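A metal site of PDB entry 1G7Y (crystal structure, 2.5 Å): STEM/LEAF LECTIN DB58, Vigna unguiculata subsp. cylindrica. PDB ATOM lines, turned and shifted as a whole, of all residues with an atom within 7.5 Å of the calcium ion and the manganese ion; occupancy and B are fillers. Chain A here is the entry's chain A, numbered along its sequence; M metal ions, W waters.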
ATOM      1  N   ASP A  85       6.994 -20.762 -15.721  1.00  0.00           N
ATOM      2  CA  ASP A  85       7.731 -19.648 -15.158  1.00  0.00           C
ATOM      3  C   ASP A  85       8.409 -18.843 -16.278  1.00  0.00           C
ATOM      4  O   ASP A  85       8.641 -17.644 -16.143  1.00  0.00           O
ATOM      5  CB  ASP A  85       8.807 -20.183 -14.208  1.00  0.00           C
ATOM      6  CG  ASP A  85       8.296 -20.287 -12.775  1.00  0.00           C
ATOM      7  OD1 ASP A  85       8.013 -19.237 -12.172  1.00  0.00           O
ATOM      8  OD2 ASP A  85       8.174 -21.419 -12.272  1.00  0.00           O
ATOM      9  N   GLY A  86       8.708 -19.505 -17.385  1.00  0.00           N
ATOM     10  CA  GLY A  86       9.338 -18.791 -18.492  1.00  0.00           C
ATOM     11  C   GLY A  86      10.485 -19.528 -19.151  1.00  0.00           C
ATOM     12  O   GLY A  86      10.849 -20.632 -18.749  1.00  0.00           O
ATOM     13  N   SER A 102      11.928 -23.377 -11.036  1.00  0.00           N
ATOM     14  CA  SER A 102      10.810 -22.450 -10.968  1.00  0.00           C
ATOM     15  C   SER A 102      11.198 -21.005 -11.314  1.00  0.00           C
ATOM     16  O   SER A 102      11.690 -20.735 -12.405  1.00  0.00           O
ATOM     17  CB  SER A 102      10.171 -22.520  -9.580  1.00  0.00           C
ATOM     18  OG  SER A 102       8.950 -21.801  -9.552  1.00  0.00           O
ATOM     19  N   GLY A 103      10.968 -20.090 -10.379  1.00  0.00           N
ATOM     20  CA  GLY A 103      11.277 -18.683 -10.604  1.00  0.00           C
ATOM     21  C   GLY A 103      12.697 -18.344 -11.012  1.00  0.00           C
ATOM     22  O   GLY A 103      12.937 -17.266 -11.561  1.00  0.00           O
ATOM     23  N   PHE A 104      13.652 -19.238 -10.767  1.00  0.00           N
ATOM     24  CA  PHE A 104      15.034 -18.971 -11.136  1.00  0.00           C
ATOM     25  C   PHE A 104      15.363 -19.440 -12.556  1.00  0.00           C
ATOM     26  O   PHE A 104      16.509 -19.320 -13.014  1.00  0.00           O
ATOM     27  CB  PHE A 104      15.984 -19.593 -10.107  1.00  0.00           C
ATOM     28  CG  PHE A 104      15.877 -18.991  -8.746  1.00  0.00           C
ATOM     29  CD1 PHE A 104      15.000 -19.518  -7.803  1.00  0.00           C
ATOM     30  CD2 PHE A 104      16.600 -17.853  -8.414  1.00  0.00           C
ATOM     31  CE1 PHE A 104      14.860 -18.928  -6.546  1.00  0.00           C
ATOM     32  CE2 PHE A 104      16.469 -17.261  -7.158  1.00  0.00           C
ATOM     33  CZ  PHE A 104      15.604 -17.794  -6.221  1.00  0.00           C
ATOM     34  N   LEU A 105      14.369 -19.982 -13.243  1.00  0.00           N
ATOM     35  CA  LEU A 105      14.505 -20.438 -14.626  1.00  0.00           C
ATOM     36  C   LEU A 105      15.652 -21.420 -14.915  1.00  0.00           C
ATOM     37  O   LEU A 105      15.996 -21.635 -16.071  1.00  0.00           O
ATOM     38  CB  LEU A 105      14.628 -19.218 -15.541  1.00  0.00           C
ATOM     39  CG  LEU A 105      13.529 -18.171 -15.361  1.00  0.00           C
ATOM     40  CD1 LEU A 105      13.749 -17.008 -16.321  1.00  0.00           C
ATOM     41  CD2 LEU A 105      12.172 -18.808 -15.613  1.00  0.00           C
ATOM     42  N   GLU A 123      15.589 -13.128 -20.367  1.00  0.00           N
ATOM     43  CA  GLU A 123      14.431 -13.898 -19.955  1.00  0.00           C
ATOM     44  C   GLU A 123      13.107 -13.424 -20.512  1.00  0.00           C
ATOM     45  O   GLU A 123      12.909 -12.250 -20.835  1.00  0.00           O
ATOM     46  CB  GLU A 123      14.326 -13.915 -18.429  1.00  0.00           C
ATOM     47  CG  GLU A 123      14.231 -12.538 -17.798  1.00  0.00           C
ATOM     48  CD  GLU A 123      13.853 -12.574 -16.334  1.00  0.00           C
ATOM     49  OE1 GLU A 123      14.582 -13.204 -15.542  1.00  0.00           O
ATOM     50  OE2 GLU A 123      12.823 -11.962 -15.974  1.00  0.00           O
ATOM     51  N   PHE A 124      12.206 -14.379 -20.629  1.00  0.00           N
ATOM     52  CA  PHE A 124      10.849 -14.144 -21.095  1.00  0.00           C
ATOM     53  C   PHE A 124      10.053 -14.753 -19.949  1.00  0.00           C
ATOM     54  O   PHE A 124       9.694 -15.938 -19.954  1.00  0.00           O
ATOM     55  CB  PHE A 124      10.666 -14.837 -22.444  1.00  0.00           C
ATOM     56  CG  PHE A 124      11.611 -14.320 -23.480  1.00  0.00           C
ATOM     57  CD1 PHE A 124      11.325 -13.147 -24.194  1.00  0.00           C
ATOM     58  CD2 PHE A 124      12.867 -14.894 -23.644  1.00  0.00           C
ATOM     59  CE1 PHE A 124      12.269 -12.567 -25.032  1.00  0.00           C
ATOM     60  CE2 PHE A 124      13.823 -14.327 -24.480  1.00  0.00           C
ATOM     61  CZ  PHE A 124      13.518 -13.155 -25.179  1.00  0.00           C
ATOM     62  N   ASP A 125       9.856 -13.903 -18.942  1.00  0.00           N
ATOM     63  CA  ASP A 125       9.203 -14.194 -17.679  1.00  0.00           C
ATOM     64  C   ASP A 125       7.673 -14.115 -17.734  1.00  0.00           C
ATOM     65  O   ASP A 125       7.111 -13.034 -17.871  1.00  0.00           O
ATOM     66  CB  ASP A 125       9.722 -13.193 -16.653  1.00  0.00           C
ATOM     67  CG  ASP A 125       9.736 -13.729 -15.257  1.00  0.00           C
ATOM     68  OD1 ASP A 125       8.818 -14.499 -14.893  1.00  0.00           O
ATOM     69  OD2 ASP A 125      10.667 -13.369 -14.508  1.00  0.00           O
ATOM     70  N   THR A 126       7.021 -15.256 -17.574  1.00  0.00           N
ATOM     71  CA  THR A 126       5.562 -15.317 -17.618  1.00  0.00           C
ATOM     72  C   THR A 126       4.898 -15.278 -16.244  1.00  0.00           C
ATOM     73  O   THR A 126       3.672 -15.157 -16.161  1.00  0.00           O
ATOM     74  CB  THR A 126       5.092 -16.570 -18.325  1.00  0.00           C
ATOM     75  OG1 THR A 126       5.635 -17.712 -17.650  1.00  0.00           O
ATOM     76  CG2 THR A 126       5.556 -16.578 -19.784  1.00  0.00           C
ATOM     77  N   PHE A 127       5.687 -15.392 -15.175  1.00  0.00           N
ATOM     78  CA  PHE A 127       5.146 -15.374 -13.822  1.00  0.00           C
ATOM     79  C   PHE A 127       5.850 -14.365 -12.944  1.00  0.00           C
ATOM     80  O   PHE A 127       7.072 -14.383 -12.798  1.00  0.00           O
ATOM     81  CB  PHE A 127       5.226 -16.763 -13.202  1.00  0.00           C
ATOM     82  CG  PHE A 127       4.838 -16.797 -11.760  1.00  0.00           C
ATOM     83  CD1 PHE A 127       5.802 -16.664 -10.759  1.00  0.00           C
ATOM     84  CD2 PHE A 127       3.500 -16.949 -11.387  1.00  0.00           C
ATOM     85  CE1 PHE A 127       5.439 -16.700  -9.410  1.00  0.00           C
ATOM     86  CE2 PHE A 127       3.128 -16.986 -10.038  1.00  0.00           C
ATOM     87  CZ  PHE A 127       4.103 -16.860  -9.043  1.00  0.00           C
ATOM     88  N   SER A 128       5.066 -13.489 -12.334  1.00  0.00           N
ATOM     89  CA  SER A 128       5.622 -12.442 -11.492  1.00  0.00           C
ATOM     90  C   SER A 128       5.971 -12.837 -10.053  1.00  0.00           C
ATOM     91  O   SER A 128       5.084 -13.035  -9.227  1.00  0.00           O
ATOM     92  CB  SER A 128       4.649 -11.262 -11.470  1.00  0.00           C
ATOM     93  OG  SER A 128       5.211 -10.163 -10.779  1.00  0.00           O
ATOM     94  N   ASN A 129       7.264 -12.881  -9.748  1.00  0.00           N
ATOM     95  CA  ASN A 129       7.759 -13.196  -8.409  1.00  0.00           C
ATOM     96  C   ASN A 129       7.829 -11.878  -7.644  1.00  0.00           C
ATOM     97  O   ASN A 129       8.752 -11.100  -7.852  1.00  0.00           O
ATOM     98  CB  ASN A 129       9.164 -13.794  -8.486  1.00  0.00           C
ATOM     99  CG  ASN A 129       9.209 -15.125  -9.202  1.00  0.00           C
ATOM    100  OD1 ASN A 129       8.842 -15.238 -10.377  1.00  0.00           O
ATOM    101  ND2 ASN A 129       9.667 -16.153  -8.505  1.00  0.00           N
ATOM    102  N   THR A 130       6.872 -11.629  -6.750  1.00  0.00           N
ATOM    103  CA  THR A 130       6.866 -10.356  -6.020  1.00  0.00           C
ATOM    104  C   THR A 130       8.187  -9.925  -5.389  1.00  0.00           C
ATOM    105  O   THR A 130       8.430  -8.727  -5.219  1.00  0.00           O
ATOM    106  CB  THR A 130       5.767 -10.331  -4.920  1.00  0.00           C
ATOM    107  OG1 THR A 130       5.837 -11.517  -4.121  1.00  0.00           O
ATOM    108  CG2 THR A 130       4.390 -10.214  -5.547  1.00  0.00           C
ATOM    109  N   TRP A 132      11.093  -9.761  -6.615  1.00  0.00           N
ATOM    110  CA  TRP A 132      12.071  -9.144  -7.480  1.00  0.00           C
ATOM    111  C   TRP A 132      11.529  -8.799  -8.865  1.00  0.00           C
ATOM    112  O   TRP A 132      12.148  -8.027  -9.587  1.00  0.00           O
ATOM    113  CB  TRP A 132      13.286 -10.067  -7.622  1.00  0.00           C
ATOM    114  CG  TRP A 132      13.003 -11.418  -8.292  1.00  0.00           C
ATOM    115  CD1 TRP A 132      12.582 -11.620  -9.589  1.00  0.00           C
ATOM    116  CD2 TRP A 132      13.111 -12.729  -7.705  1.00  0.00           C
ATOM    117  NE1 TRP A 132      12.437 -12.965  -9.834  1.00  0.00           N
ATOM    118  CE2 TRP A 132      12.756 -13.673  -8.700  1.00  0.00           C
ATOM    119  CE3 TRP A 132      13.494 -13.200  -6.441  1.00  0.00           C
ATOM    120  CZ2 TRP A 132      12.758 -15.054  -8.465  1.00  0.00           C
ATOM    121  CZ3 TRP A 132      13.496 -14.581  -6.206  1.00  0.00           C
ATOM    122  CH2 TRP A 132      13.135 -15.486  -7.221  1.00  0.00           C
ATOM    123  N   ASP A 133      10.402  -9.382  -9.237  1.00  0.00           N
ATOM    124  CA  ASP A 133       9.833  -9.109 -10.547  1.00  0.00           C
ATOM    125  C   ASP A 133       8.912  -7.903 -10.651  1.00  0.00           C
ATOM    126  O   ASP A 133       8.443  -7.358  -9.645  1.00  0.00           O
ATOM    127  CB  ASP A 133       9.018 -10.302 -11.069  1.00  0.00           C
ATOM    128  CG  ASP A 133       9.885 -11.393 -11.651  1.00  0.00           C
ATOM    129  OD1 ASP A 133      11.005 -11.091 -12.119  1.00  0.00           O
ATOM    130  OD2 ASP A 133       9.411 -12.560 -11.663  1.00  0.00           O
ATOM    131  N   PRO A 134       8.674  -7.449 -11.887  1.00  0.00           N
ATOM    132  CA  PRO A 134       7.787  -6.313 -12.124  1.00  0.00           C
ATOM    133  C   PRO A 134       6.392  -6.937 -12.034  1.00  0.00           C
ATOM    134  O   PRO A 134       6.264  -8.158 -11.961  1.00  0.00           O
ATOM    135  CB  PRO A 134       8.134  -5.910 -13.560  1.00  0.00           C
ATOM    136  CG  PRO A 134       9.551  -6.326 -13.692  1.00  0.00           C
ATOM    137  CD  PRO A 134       9.546  -7.681 -13.046  1.00  0.00           C
ATOM    138  N   SER A 136       3.849  -7.232 -14.334  1.00  0.00           N
ATOM    139  CA  SER A 136       3.374  -8.064 -15.428  1.00  0.00           C
ATOM    140  C   SER A 136       4.431  -8.946 -16.058  1.00  0.00           C
ATOM    141  O   SER A 136       5.595  -8.910 -15.661  1.00  0.00           O
ATOM    142  CB  SER A 136       2.766  -7.160 -16.511  1.00  0.00           C
ATOM    143  OG  SER A 136       3.738  -6.239 -16.983  1.00  0.00           O
ATOM    144  N   ARG A 137       4.007  -9.747 -17.036  1.00  0.00           N
ATOM    145  CA  ARG A 137       4.926 -10.612 -17.758  1.00  0.00           C
ATOM    146  C   ARG A 137       5.916  -9.654 -18.407  1.00  0.00           C
ATOM    147  O   ARG A 137       5.542  -8.550 -18.795  1.00  0.00           O
ATOM    148  CB  ARG A 137       4.167 -11.427 -18.799  1.00  0.00           C
ATOM    149  CG  ARG A 137       3.131 -12.353 -18.182  1.00  0.00           C
ATOM    150  CD  ARG A 137       2.696 -13.436 -19.156  1.00  0.00           C
ATOM    151  NE  ARG A 137       1.632 -14.258 -18.596  1.00  0.00           N
ATOM    152  CZ  ARG A 137       0.378 -13.843 -18.439  1.00  0.00           C
ATOM    153  NH1 ARG A 137       0.028 -12.619 -18.816  1.00  0.00           N
ATOM    154  NH2 ARG A 137      -0.537 -14.656 -17.919  1.00  0.00           N
ATOM    155  N   HIS A 138       7.162 -10.074 -18.542  1.00  0.00           N
ATOM    156  CA  HIS A 138       8.154  -9.166 -19.077  1.00  0.00           C
ATOM    157  C   HIS A 138       9.352  -9.837 -19.732  1.00  0.00           C
ATOM    158  O   HIS A 138       9.578 -11.036 -19.570  1.00  0.00           O
ATOM    159  CB  HIS A 138       8.680  -8.320 -17.928  1.00  0.00           C
ATOM    160  CG  HIS A 138       9.137  -9.132 -16.755  1.00  0.00           C
ATOM    161  ND1 HIS A 138       8.261  -9.754 -15.884  1.00  0.00           N
ATOM    162  CD2 HIS A 138      10.380  -9.508 -16.352  1.00  0.00           C
ATOM    163  CE1 HIS A 138       8.945 -10.473 -15.014  1.00  0.00           C
ATOM    164  NE2 HIS A 138      10.230 -10.342 -15.269  1.00  0.00           N
ATOM    165  N   ILE A 139      10.107  -9.032 -20.462  1.00  0.00           N
ATOM    166  CA  ILE A 139      11.344  -9.464 -21.094  1.00  0.00           C
ATOM    167  C   ILE A 139      12.372  -8.808 -20.188  1.00  0.00           C
ATOM    168  O   ILE A 139      12.188  -7.662 -19.779  1.00  0.00           O
ATOM    169  CB  ILE A 139      11.533  -8.862 -22.496  1.00  0.00           C
ATOM    170  CG1 ILE A 139      10.404  -9.304 -23.416  1.00  0.00           C
ATOM    171  CG2 ILE A 139      12.877  -9.319 -23.063  1.00  0.00           C
ATOM    172  CD1 ILE A 139      10.461  -8.614 -24.770  1.00  0.00           C
ATOM    173  N   GLY A 140      13.435  -9.516 -19.857  1.00  0.00           N
ATOM    174  CA  GLY A 140      14.429  -8.913 -18.985  1.00  0.00           C
ATOM    175  C   GLY A 140      15.851  -9.336 -19.273  1.00  0.00           C
ATOM    176  O   GLY A 140      16.100 -10.411 -19.815  1.00  0.00           O
ATOM    177  N   ASP A 142      19.199 -10.351 -17.560  1.00  0.00           N
ATOM    178  CA  ASP A 142      19.735 -10.830 -16.299  1.00  0.00           C
ATOM    179  C   ASP A 142      21.250 -10.973 -16.328  1.00  0.00           C
ATOM    180  O   ASP A 142      21.801 -11.696 -17.154  1.00  0.00           O
ATOM    181  CB  ASP A 142      19.132 -12.189 -15.945  1.00  0.00           C
ATOM    182  CG  ASP A 142      17.615 -12.154 -15.858  1.00  0.00           C
ATOM    183  OD1 ASP A 142      17.027 -11.051 -15.812  1.00  0.00           O
ATOM    184  OD2 ASP A 142      17.002 -13.248 -15.820  1.00  0.00           O
ATOM    185  N   ILE A 146      18.819 -13.152 -10.805  1.00  0.00           N
ATOM    186  CA  ILE A 146      17.510 -13.294 -11.398  1.00  0.00           C
ATOM    187  C   ILE A 146      16.806 -11.945 -11.377  1.00  0.00           C
ATOM    188  O   ILE A 146      15.784 -11.773 -12.041  1.00  0.00           O
ATOM    189  CB  ILE A 146      16.669 -14.347 -10.653  1.00  0.00           C
ATOM    190  CG1 ILE A 146      15.402 -14.643 -11.469  1.00  0.00           C
ATOM    191  CG2 ILE A 146      16.327 -13.861  -9.256  1.00  0.00           C
ATOM    192  CD1 ILE A 146      15.662 -15.311 -12.788  1.00  0.00           C
ATOM    193  N   LYS A 147      17.332 -10.993 -10.615  1.00  0.00           N
ATOM    194  CA  LYS A 147      16.723  -9.661 -10.557  1.00  0.00           C
ATOM    195  C   LYS A 147      17.246  -8.851 -11.739  1.00  0.00           C
ATOM    196  O   LYS A 147      18.307  -8.250 -11.647  1.00  0.00           O
ATOM    197  CB  LYS A 147      17.103  -8.950  -9.237  1.00  0.00           C
ATOM    198  CG  LYS A 147      16.347  -7.640  -8.923  1.00  0.00           C
ATOM    199  CD  LYS A 147      17.094  -6.870  -7.827  1.00  0.00           C
ATOM    200  CE  LYS A 147      16.181  -6.243  -6.793  1.00  0.00           C
ATOM    201  NZ  LYS A 147      15.336  -5.141  -7.327  1.00  0.00           N
ATOM    202  N   SER A 148      16.501  -8.851 -12.850  1.00  0.00           N
ATOM    203  CA  SER A 148      16.893  -8.132 -14.081  1.00  0.00           C
ATOM    204  C   SER A 148      17.425  -6.726 -13.810  1.00  0.00           C
ATOM    205  O   SER A 148      16.973  -6.034 -12.896  1.00  0.00           O
ATOM    206  CB  SER A 148      15.712  -8.004 -15.057  1.00  0.00           C
ATOM    207  OG  SER A 148      15.175  -9.260 -15.441  1.00  0.00           O
ATOM    208  N   THR A 151      13.958  -4.257 -17.538  1.00  0.00           N
ATOM    209  CA  THR A 151      12.880  -5.085 -18.062  1.00  0.00           C
ATOM    210  C   THR A 151      11.947  -4.249 -18.921  1.00  0.00           C
ATOM    211  O   THR A 151      12.058  -3.033 -18.957  1.00  0.00           O
ATOM    212  CB  THR A 151      12.044  -5.702 -16.928  1.00  0.00           C
ATOM    213  OG1 THR A 151      11.405  -4.662 -16.180  1.00  0.00           O
ATOM    214  CG2 THR A 151      12.935  -6.504 -15.987  1.00  0.00           C
HETATM  215 CA    CA M   1       9.366 -14.532 -12.594  1.00  0.00          CA
HETATM  216 MN    MN M   2      11.688 -11.546 -14.185  1.00  0.00          MN
HETATM  217  O   HOH W   1      12.732  -9.892 -13.640  1.00  0.00           O
HETATM  218  O   HOH W   2      13.190 -12.704 -13.123  1.00  0.00           O
HETATM  219  O   HOH W   3      11.588 -14.850 -12.016  1.00  0.00           O
HETATM  220  O   HOH W   4       8.898 -16.686 -13.348  1.00  0.00           O
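OD2 of Asp 142 sits close to OE1 of Glu 123 (2.4 Å). The backbone NH (N) of Glu 123 sits at hydrogen-bond distance from the backbone carbonyl oxygen (O) of Gly 140. A ring nitrogen (ND1) of His 138 is in hydrogen-bond range of the backbone carbonyl oxygen of Ser 136. The side-chain carboxylate (OD1) of Asp 133 sits close to the indole nitrogen (NE1) of Trp 132 (3.3 Å).
Four residues have an atom within 4 Å of the calcium ion: Asp 125, Phe 127, Asn 129 and Asp 133. Along chain A the residues within 4 Å of the calcium ion span positions 125 to 133.
Within 4 Å of the manganese ion: Glu 123, Asp 125, Asp 133 and His 138. Along chain A the residues within 4 Å of the manganese ion span positions 123 to 138. The nearest printed residue that does not touch the manganese ion is Ser 148 (4.4 Å).
The calcium ion is bound by the side-chain carboxylate (OD2) of Asp 133 (2.2 Å), the backbone carbonyl oxygen (O) of Phe 127 (2.3 Å), water W3 (2.3 Å), water W4 (2.3 Å), the side-chain carboxylate (OD1) of Asp 125 (2.4 Å), the side-chain amide oxygen (OD1) of Asn 129 (2.4 Å) and the side-chain carboxylate (OD2) of Asp 125 (2.6 Å).
The manganese ion is bound by water W1 (2.0 Å), OD2 of Asp 125 (2.1 Å), OE2 of Glu 123 (2.2 Å), water W2 (2.2 Å), NE2 of His 138 (2.2 Å) and OD1 of Asp 133 (2.2 Å). The manganese ion has six donor atoms within binding distance.
Water W3 lies within hydrogen-bond range of the backbone carbonyl oxygen (O) of Gly 103 (2.8 Å) and the indole nitrogen (NE1) of Trp 132 (3.0 Å). Water W2 lies within hydrogen-bond range of OE1 of Glu 123, O of Ile 146 and NE1 of Trp 132.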
